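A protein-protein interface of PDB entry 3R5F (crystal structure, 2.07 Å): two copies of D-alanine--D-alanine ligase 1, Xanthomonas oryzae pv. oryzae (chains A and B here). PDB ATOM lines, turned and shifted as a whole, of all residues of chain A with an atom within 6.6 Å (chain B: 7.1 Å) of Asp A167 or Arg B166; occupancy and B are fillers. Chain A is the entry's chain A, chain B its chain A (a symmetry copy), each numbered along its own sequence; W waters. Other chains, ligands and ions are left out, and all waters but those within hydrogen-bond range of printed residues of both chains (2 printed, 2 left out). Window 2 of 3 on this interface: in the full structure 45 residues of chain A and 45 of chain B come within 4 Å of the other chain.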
ATOM      1  N   LYS A 162     -13.309  -9.112  -8.490  1.00  0.00           N
ATOM      2  CA  LYS A 162     -14.249  -8.138  -7.833  1.00  0.00           C
ATOM      3  C   LYS A 162     -15.327  -7.643  -8.806  1.00  0.00           C
ATOM      4  O   LYS A 162     -16.527  -7.529  -8.416  1.00  0.00           O
ATOM      5  CB  LYS A 162     -13.486  -6.922  -7.269  1.00  0.00           C
ATOM      6  CG  LYS A 162     -12.620  -7.207  -5.959  1.00  0.00           C
ATOM      7  CD  LYS A 162     -11.857  -5.833  -5.651  1.00  0.00           C
ATOM      8  CE  LYS A 162     -11.797  -5.343  -4.217  1.00  0.00           C
ATOM      9  NZ  LYS A 162     -12.976  -5.020  -3.446  1.00  0.00           N
ATOM     10  N   ARG A 163     -14.929  -7.377 -10.074  1.00  0.00           N
ATOM     11  CA  ARG A 163     -15.920  -6.908 -11.073  1.00  0.00           C
ATOM     12  C   ARG A 163     -16.909  -8.034 -11.382  1.00  0.00           C
ATOM     13  O   ARG A 163     -18.128  -7.750 -11.590  1.00  0.00           O
ATOM     14  CB  ARG A 163     -15.299  -6.361 -12.387  1.00  0.00           C
ATOM     15  CG  ARG A 163     -14.386  -5.139 -12.179  1.00  0.00           C
ATOM     16  CD  ARG A 163     -13.902  -4.452 -13.462  1.00  0.00           C
ATOM     17  NE  ARG A 163     -12.603  -4.995 -13.868  1.00  0.00           N
ATOM     18  CZ  ARG A 163     -12.301  -5.470 -15.065  1.00  0.00           C
ATOM     19  NH1 ARG A 163     -13.226  -5.519 -16.053  1.00  0.00           N
ATOM     20  NH2 ARG A 163     -11.064  -5.895 -15.280  1.00  0.00           N
ATOM     21  N   VAL A 164     -16.383  -9.273 -11.456  1.00  0.00           N
ATOM     22  CA  VAL A 164     -17.255 -10.432 -11.749  1.00  0.00           C
ATOM     23  C   VAL A 164     -18.186 -10.677 -10.544  1.00  0.00           C
ATOM     24  O   VAL A 164     -19.407 -10.927 -10.721  1.00  0.00           O
ATOM     25  CB  VAL A 164     -16.526 -11.721 -12.126  1.00  0.00           C
ATOM     26  CG1 VAL A 164     -17.575 -12.911 -12.225  1.00  0.00           C
ATOM     27  CG2 VAL A 164     -15.880 -11.566 -13.539  1.00  0.00           C
ATOM     28  N   LEU A 165     -17.605 -10.630  -9.348  1.00  0.00           N
ATOM     29  CA  LEU A 165     -18.377 -10.770  -8.086  1.00  0.00           C
ATOM     30  C   LEU A 165     -19.454  -9.716  -7.964  1.00  0.00           C
ATOM     31  O   LEU A 165     -20.609 -10.023  -7.591  1.00  0.00           O
ATOM     32  CB  LEU A 165     -17.448 -10.715  -6.846  1.00  0.00           C
ATOM     33  CG  LEU A 165     -16.568 -11.983  -6.863  1.00  0.00           C
ATOM     34  CD1 LEU A 165     -15.579 -11.896  -5.651  1.00  0.00           C
ATOM     35  CD2 LEU A 165     -17.432 -13.268  -6.712  1.00  0.00           C
ATOM     36  N   ARG A 166     -19.054  -8.476  -8.278  1.00  0.00           N
ATOM     37  CA  ARG A 166     -19.874  -7.289  -8.165  1.00  0.00           C
ATOM     38  C   ARG A 166     -21.092  -7.475  -9.041  1.00  0.00           C
ATOM     39  O   ARG A 166     -22.201  -7.057  -8.652  1.00  0.00           O
ATOM     40  CB  ARG A 166     -19.063  -6.026  -8.645  1.00  0.00           C
ATOM     41  CG  ARG A 166     -19.853  -4.789  -8.934  1.00  0.00           C
ATOM     42  CD  ARG A 166     -18.998  -3.476  -8.947  1.00  0.00           C
ATOM     43  NE  ARG A 166     -18.170  -3.323 -10.162  1.00  0.00           N
ATOM     44  CZ  ARG A 166     -17.192  -2.435 -10.279  1.00  0.00           C
ATOM     45  NH1 ARG A 166     -16.834  -1.704  -9.240  1.00  0.00           N
ATOM     46  NH2 ARG A 166     -16.515  -2.340 -11.417  1.00  0.00           N
ATOM     47  N   ASP A 167     -20.862  -8.011 -10.246  1.00  0.00           N
ATOM     48  CA  ASP A 167     -21.880  -8.164 -11.257  1.00  0.00           C
ATOM     49  C   ASP A 167     -22.852  -9.269 -10.827  1.00  0.00           C
ATOM     50  O   ASP A 167     -24.027  -9.240 -11.173  1.00  0.00           O
ATOM     51  CB  ASP A 167     -21.219  -8.542 -12.592  1.00  0.00           C
ATOM     52  CG  ASP A 167     -22.215  -8.947 -13.664  1.00  0.00           C
ATOM     53  OD1 ASP A 167     -22.783  -8.031 -14.284  1.00  0.00           O
ATOM     54  OD2 ASP A 167     -22.412 -10.183 -13.904  1.00  0.00           O
ATOM     55  N   ALA A 168     -22.359 -10.250 -10.091  1.00  0.00           N
ATOM     56  CA  ALA A 168     -23.216 -11.323  -9.607  1.00  0.00           C
ATOM     57  C   ALA A 168     -23.955 -10.879  -8.295  1.00  0.00           C
ATOM     58  O   ALA A 168     -24.489 -11.730  -7.560  1.00  0.00           O
ATOM     59  CB  ALA A 168     -22.372 -12.500  -9.296  1.00  0.00           C
ATOM     60  N   ARG A 169     -23.906  -9.575  -8.013  1.00  0.00           N
ATOM     61  CA  ARG A 169     -24.547  -8.938  -6.868  1.00  0.00           C
ATOM     62  C   ARG A 169     -24.059  -9.501  -5.581  1.00  0.00           C
ATOM     63  O   ARG A 169     -24.854  -9.627  -4.656  1.00  0.00           O
ATOM     64  CB  ARG A 169     -26.098  -9.082  -6.864  1.00  0.00           C
ATOM     65  CG  ARG A 169     -26.836  -8.905  -8.201  1.00  0.00           C
ATOM     66  CD  ARG A 169     -26.863  -7.453  -8.627  1.00  0.00           C
ATOM     67  NE  ARG A 169     -25.806  -7.224  -9.598  1.00  0.00           N
ATOM     68  CZ  ARG A 169     -25.865  -6.360 -10.616  1.00  0.00           C
ATOM     69  NH1 ARG A 169     -26.959  -5.606 -10.804  1.00  0.00           N
ATOM     70  NH2 ARG A 169     -24.822  -6.264 -11.448  1.00  0.00           N
ATOM     71  N   LEU A 170     -22.759  -9.805  -5.504  1.00  0.00           N
ATOM     72  CA  LEU A 170     -22.119 -10.060  -4.235  1.00  0.00           C
ATOM     73  C   LEU A 170     -21.316  -8.799  -3.856  1.00  0.00           C
ATOM     74  O   LEU A 170     -20.841  -8.100  -4.746  1.00  0.00           O
ATOM     75  CB  LEU A 170     -21.242 -11.310  -4.363  1.00  0.00           C
ATOM     76  CG  LEU A 170     -21.996 -12.587  -4.760  1.00  0.00           C
ATOM     77  CD1 LEU A 170     -21.144 -13.716  -5.378  1.00  0.00           C
ATOM     78  CD2 LEU A 170     -22.759 -13.120  -3.504  1.00  0.00           C
ATOM     79  N   ASP B 159     -20.360 -15.948 -21.896  1.00  0.00           N
ATOM     80  CA  ASP B 159     -21.048 -15.688 -20.690  1.00  0.00           C
ATOM     81  C   ASP B 159     -20.238 -14.765 -19.758  1.00  0.00           C
ATOM     82  O   ASP B 159     -20.704 -13.729 -19.337  1.00  0.00           O
ATOM     83  CB  ASP B 159     -21.304 -17.005 -19.976  1.00  0.00           C
ATOM     84  CG  ASP B 159     -21.777 -16.821 -18.532  1.00  0.00           C
ATOM     85  OD1 ASP B 159     -22.661 -15.987 -18.262  1.00  0.00           O
ATOM     86  OD2 ASP B 159     -21.270 -17.532 -17.687  1.00  0.00           O
ATOM     87  N   MET B 160     -19.019 -15.160 -19.453  1.00  0.00           N
ATOM     88  CA  MET B 160     -18.179 -14.340 -18.559  1.00  0.00           C
ATOM     89  C   MET B 160     -17.927 -12.957 -19.257  1.00  0.00           C
ATOM     90  O   MET B 160     -18.006 -11.928 -18.615  1.00  0.00           O
ATOM     91  CB  MET B 160     -16.874 -15.113 -18.324  1.00  0.00           C
ATOM     92  CG  MET B 160     -15.834 -14.439 -17.496  1.00  0.00           C
ATOM     93  SD  MET B 160     -16.419 -14.384 -15.806  1.00  0.00           S
ATOM     94  CE  MET B 160     -16.166 -16.083 -15.276  1.00  0.00           C
ATOM     95  N   ALA B 161     -17.602 -12.961 -20.544  1.00  0.00           N
ATOM     96  CA  ALA B 161     -17.391 -11.703 -21.322  1.00  0.00           C
ATOM     97  C   ALA B 161     -18.529 -10.709 -21.258  1.00  0.00           C
ATOM     98  O   ALA B 161     -18.277  -9.583 -20.910  1.00  0.00           O
ATOM     99  CB  ALA B 161     -17.033 -11.989 -22.805  1.00  0.00           C
ATOM    100  N   LYS B 162     -19.771 -11.151 -21.508  1.00  0.00           N
ATOM    101  CA  LYS B 162     -20.999 -10.291 -21.375  1.00  0.00           C
ATOM    102  C   LYS B 162     -21.157  -9.741 -19.952  1.00  0.00           C
ATOM    103  O   LYS B 162     -21.516  -8.539 -19.775  1.00  0.00           O
ATOM    104  CB  LYS B 162     -22.271 -11.076 -21.754  1.00  0.00           C
ATOM    105  CG  LYS B 162     -22.455 -11.368 -23.312  1.00  0.00           C
ATOM    106  CD  LYS B 162     -23.771 -12.274 -23.419  1.00  0.00           C
ATOM    107  CE  LYS B 162     -24.779 -11.962 -24.507  1.00  0.00           C
ATOM    108  NZ  LYS B 162     -25.477 -10.700 -24.595  1.00  0.00           N
ATOM    109  N   ARG B 163     -20.869 -10.587 -18.934  1.00  0.00           N
ATOM    110  CA  ARG B 163     -20.985 -10.119 -17.531  1.00  0.00           C
ATOM    111  C   ARG B 163     -19.916  -9.063 -17.253  1.00  0.00           C
ATOM    112  O   ARG B 163     -20.195  -8.080 -16.499  1.00  0.00           O
ATOM    113  CB  ARG B 163     -20.918 -11.250 -16.468  1.00  0.00           C
ATOM    114  CG  ARG B 163     -22.043 -12.292 -16.600  1.00  0.00           C
ATOM    115  CD  ARG B 163     -22.126 -13.318 -15.462  1.00  0.00           C
ATOM    116  NE  ARG B 163     -21.362 -14.520 -15.807  1.00  0.00           N
ATOM    117  CZ  ARG B 163     -20.429 -15.087 -15.059  1.00  0.00           C
ATOM    118  NH1 ARG B 163     -20.073 -14.560 -13.865  1.00  0.00           N
ATOM    119  NH2 ARG B 163     -19.855 -16.195 -15.505  1.00  0.00           N
ATOM    120  N   VAL B 164     -18.709  -9.288 -17.809  1.00  0.00           N
ATOM    121  CA  VAL B 164     -17.604  -8.325 -17.601  1.00  0.00           C
ATOM    122  C   VAL B 164     -17.933  -7.017 -18.348  1.00  0.00           C
ATOM    123  O   VAL B 164     -17.734  -5.901 -17.797  1.00  0.00           O
ATOM    124  CB  VAL B 164     -16.216  -8.827 -17.995  1.00  0.00           C
ATOM    125  CG1 VAL B 164     -15.175  -7.631 -17.893  1.00  0.00           C
ATOM    126  CG2 VAL B 164     -15.747  -9.924 -16.987  1.00  0.00           C
ATOM    127  N   LEU B 165     -18.399  -7.161 -19.585  1.00  0.00           N
ATOM    128  CA  LEU B 165     -18.832  -6.002 -20.409  1.00  0.00           C
ATOM    129  C   LEU B 165     -19.933  -5.213 -19.737  1.00  0.00           C
ATOM    130  O   LEU B 165     -19.895  -3.963 -19.704  1.00  0.00           O
ATOM    131  CB  LEU B 165     -19.294  -6.452 -21.818  1.00  0.00           C
ATOM    132  CG  LEU B 165     -18.054  -6.976 -22.574  1.00  0.00           C
ATOM    133  CD1 LEU B 165     -18.529  -7.496 -23.972  1.00  0.00           C
ATOM    134  CD2 LEU B 165     -17.008  -5.845 -22.791  1.00  0.00           C
ATOM    135  N   ARG B 166     -20.911  -5.965 -19.213  1.00  0.00           N
ATOM    136  CA  ARG B 166     -22.110  -5.445 -18.591  1.00  0.00           C
ATOM    137  C   ARG B 166     -21.696  -4.580 -17.423  1.00  0.00           C
ATOM    138  O   ARG B 166     -22.323  -3.530 -17.180  1.00  0.00           O
ATOM    139  CB  ARG B 166     -23.011  -6.633 -18.079  1.00  0.00           C
ATOM    140  CG  ARG B 166     -24.094  -6.286 -17.107  1.00  0.00           C
ATOM    141  CD  ARG B 166     -25.220  -7.370 -16.996  1.00  0.00           C
ATOM    142  NE  ARG B 166     -24.813  -8.567 -16.231  1.00  0.00           N
ATOM    143  CZ  ARG B 166     -25.499  -9.703 -16.220  1.00  0.00           C
ATOM    144  NH1 ARG B 166     -26.547  -9.848 -17.007  1.00  0.00           N
ATOM    145  NH2 ARG B 166     -25.081 -10.722 -15.481  1.00  0.00           N
ATOM    146  N   ASP B 167     -20.711  -5.071 -16.659  1.00  0.00           N
ATOM    147  CA  ASP B 167     -20.256  -4.441 -15.444  1.00  0.00           C
ATOM    148  C   ASP B 167     -19.496  -3.159 -15.797  1.00  0.00           C
ATOM    149  O   ASP B 167     -19.483  -2.205 -15.028  1.00  0.00           O
ATOM    150  CB  ASP B 167     -19.330  -5.406 -14.687  1.00  0.00           C
ATOM    151  CG  ASP B 167     -18.619  -4.760 -13.511  1.00  0.00           C
ATOM    152  OD1 ASP B 167     -19.259  -4.653 -12.450  1.00  0.00           O
ATOM    153  OD2 ASP B 167     -17.410  -4.380 -13.639  1.00  0.00           O
ATOM    154  N   ALA B 168     -18.847  -3.143 -16.949  1.00  0.00           N
ATOM    155  CA  ALA B 168     -18.126  -1.954 -17.383  1.00  0.00           C
ATOM    156  C   ALA B 168     -19.111  -0.942 -18.068  1.00  0.00           C
ATOM    157  O   ALA B 168     -18.666  -0.015 -18.770  1.00  0.00           O
ATOM    158  CB  ALA B 168     -17.101  -2.357 -18.374  1.00  0.00           C
ATOM    159  N   ARG B 169     -20.411  -1.186 -17.894  1.00  0.00           N
ATOM    160  CA  ARG B 169     -21.499  -0.363 -18.410  1.00  0.00           C
ATOM    161  C   ARG B 169     -21.450  -0.253 -19.891  1.00  0.00           C
ATOM    162  O   ARG B 169     -21.766   0.810 -20.412  1.00  0.00           O
ATOM    163  CB  ARG B 169     -21.496   1.090 -17.850  1.00  0.00           C
ATOM    164  CG  ARG B 169     -21.193   1.281 -16.355  1.00  0.00           C
ATOM    165  CD  ARG B 169     -22.356   0.836 -15.496  1.00  0.00           C
ATOM    166  NE  ARG B 169     -22.095  -0.507 -15.003  1.00  0.00           N
ATOM    167  CZ  ARG B 169     -22.490  -0.988 -13.821  1.00  0.00           C
ATOM    168  NH1 ARG B 169     -23.197  -0.220 -12.977  1.00  0.00           N
ATOM    169  NH2 ARG B 169     -22.164  -2.242 -13.488  1.00  0.00           N
ATOM    170  N   LEU B 170     -21.095  -1.349 -20.571  1.00  0.00           N
ATOM    171  CA  LEU B 170     -21.310  -1.454 -21.996  1.00  0.00           C
ATOM    172  C   LEU B 170     -22.546  -2.348 -22.217  1.00  0.00           C
ATOM    173  O   LEU B 170     -22.796  -3.237 -21.409  1.00  0.00           O
ATOM    174  CB  LEU B 170     -20.042  -2.017 -22.648  1.00  0.00           C
ATOM    175  CG  LEU B 170     -18.779  -1.170 -22.436  1.00  0.00           C
ATOM    176  CD1 LEU B 170     -17.431  -1.900 -22.619  1.00  0.00           C
ATOM    177  CD2 LEU B 170     -18.849   0.068 -23.389  1.00  0.00           C
ATOM    178  N   ALA B 171     -23.319  -2.068 -23.262  1.00  0.00           N
ATOM    179  CA  ALA B 171     -24.592  -2.705 -23.511  1.00  0.00           C
ATOM    180  C   ALA B 171     -24.265  -4.026 -24.172  1.00  0.00           C
ATOM    181  O   ALA B 171     -23.366  -4.055 -25.029  1.00  0.00           O
ATOM    182  CB  ALA B 171     -25.387  -1.883 -24.472  1.00  0.00           C
ATOM    183  N   VAL B 172     -24.914  -5.106 -23.757  1.00  0.00           N
ATOM    184  CA  VAL B 172     -24.722  -6.415 -24.466  1.00  0.00           C
ATOM    185  C   VAL B 172     -26.139  -6.925 -24.625  1.00  0.00           C
ATOM    186  O   VAL B 172     -27.002  -6.388 -23.947  1.00  0.00           O
ATOM    187  CB  VAL B 172     -23.864  -7.434 -23.691  1.00  0.00           C
ATOM    188  CG1 VAL B 172     -22.403  -6.908 -23.563  1.00  0.00           C
ATOM    189  CG2 VAL B 172     -24.478  -7.693 -22.325  1.00  0.00           C
ATOM    190  N   ALA B 173     -26.407  -7.883 -25.498  1.00  0.00           N
ATOM    191  CA  ALA B 173     -27.820  -8.423 -25.571  1.00  0.00           C
ATOM    192  C   ALA B 173     -28.267  -8.963 -24.231  1.00  0.00           C
ATOM    193  O   ALA B 173     -27.574  -9.784 -23.607  1.00  0.00           O
ATOM    194  CB  ALA B 173     -27.876  -9.520 -26.559  1.00  0.00           C
ATOM    195  N   PRO B 174     -29.461  -8.591 -23.785  1.00  0.00           N
ATOM    196  CA  PRO B 174     -29.963  -9.284 -22.604  1.00  0.00           C
ATOM    197  C   PRO B 174     -30.066 -10.853 -22.815  1.00  0.00           C
ATOM    198  O   PRO B 174     -30.215 -11.307 -23.913  1.00  0.00           O
ATOM    199  CB  PRO B 174     -31.343  -8.646 -22.372  1.00  0.00           C
ATOM    200  CG  PRO B 174     -31.599  -7.806 -23.639  1.00  0.00           C
ATOM    201  CD  PRO B 174     -30.300  -7.452 -24.197  1.00  0.00           C
ATOM    202  N   PHE B 175     -29.905 -11.623 -21.753  1.00  0.00           N
ATOM    203  CA  PHE B 175     -29.650 -13.051 -21.861  1.00  0.00           C
ATOM    204  C   PHE B 175     -29.752 -13.781 -20.548  1.00  0.00           C
ATOM    205  O   PHE B 175     -29.664 -13.192 -19.460  1.00  0.00           O
ATOM    206  CB  PHE B 175     -28.223 -13.306 -22.417  1.00  0.00           C
ATOM    207  CG  PHE B 175     -27.138 -13.071 -21.427  1.00  0.00           C
ATOM    208  CD1 PHE B 175     -26.488 -14.149 -20.814  1.00  0.00           C
ATOM    209  CD2 PHE B 175     -26.732 -11.759 -21.113  1.00  0.00           C
ATOM    210  CE1 PHE B 175     -25.442 -13.940 -19.922  1.00  0.00           C
ATOM    211  CE2 PHE B 175     -25.671 -11.543 -20.237  1.00  0.00           C
ATOM    212  CZ  PHE B 175     -25.029 -12.619 -19.638  1.00  0.00           C
HETATM  213  O   HOH W   1     -15.913  -4.661 -15.931  1.00  0.00           O
HETATM  214  O   HOH W   2     -21.127 -12.252 -12.624  1.00  0.00           O
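NE of Arg B166 is in salt-bridge range of OD1 of Asp A167 (2.9 Å). The side-chain carboxylate (OD1) of Asp A167 lies close to the backbone carbonyl oxygen (O) of Arg B163, 3.4 Å away. The guanidinium group of Arg A166 is in salt-bridge range of the side-chain carboxylate of Asp B167, at 2.9 Å. O of Arg A163 lies close to OD1 of Asp B167 (3.4 Å).
OD1 of Asp A167 is in salt-bridge range of NH2 of Arg A169 (3.9 Å). OD2 of Asp B159 is in salt-bridge range of NH2 of Arg B163 (2.9 Å). OD1 of Asp B167 lies within salt-bridge range of NH2 of Arg B169 (3.9 Å).
CG1 of Val B164 touches NH1 of Arg A163 (3.4 Å). Val A164 touches Met B160 (CG2 to SD, 3.7 Å). Val A164 touches Arg B163 (CG1 to NH1, 3.4 Å). CG2 of Val B164 touches CG2 of Val A164, at 3.8 Å.
Of chain B, only Arg B163 and Arg B166 come within 4 Å of Asp A167. Of chain A, only Asp A167 (2.9 Å) comes within 4 Å of Arg B166. Of the printed residues of chain A, Met B160 touches Val A164 (3.7 Å). Printed residues of chain B within 4 Å of Val A164: Met B160 (3.7 Å), Arg B163 (3.4 Å) and Val B164 (3.8 Å). Of the printed residues of chain B, Arg A163 touches Val B164 (3.4 Å) and Asp B167 (3.2 Å). Leu A170 touches none of the printed residues of chain B. The nearest residue of chain B that does not touch Asp A167 is Asp B167 (4.2 Å).
Of the 9 printed residues of chain A, 4 touch a printed residue of chain B. Printed residues of chain A that touch a printed residue of chain B: Arg A163, Val A164, Arg A166 and Asp A167. Of the 17 printed residues of chain B, 5 touch a printed residue of chain A. Printed residues of chain B that touch a printed residue of chain A: Met B160, Arg B163, Val B164, Arg B166 and Asp B167. Among the printed residues, Asp or Glu carboxylates within 4 Å of a Lys or Arg side-chain nitrogen of the other chain: Arg A166 with Asp B167 (2.9 Å) and Asp A167 with Arg B166 (2.9 Å).
Arg A163 touches Val B164, and with the chains exchanged Val A164 touches Arg B163. Arg A163 touches Asp B167, and with the chains exchanged Asp A167 touches Arg B163. Val B164 touches its own counterpart, Val A164. Arg A166 touches Asp B167, and with the chains exchanged Asp A167 touches Arg B166. Positions printed for both chains: 162, 163, 164, 165, 166, 167, 168, 169 and 170. Of the 8 pairs that touch across the chains among the printed residues, 7 have their exchanged pair printed and touching as well.
Water W2 lies within hydrogen-bond range of OD2 of Asp A167, NH1 of Arg B163, O of Val A164 and N of Ala A168. Water W1 lies within hydrogen-bond range of the side-chain carboxylate of Asp B167, the guanidinium group of Arg A163, the backbone carbonyl oxygen of Val B164 and the backbone NH of Ala B168.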
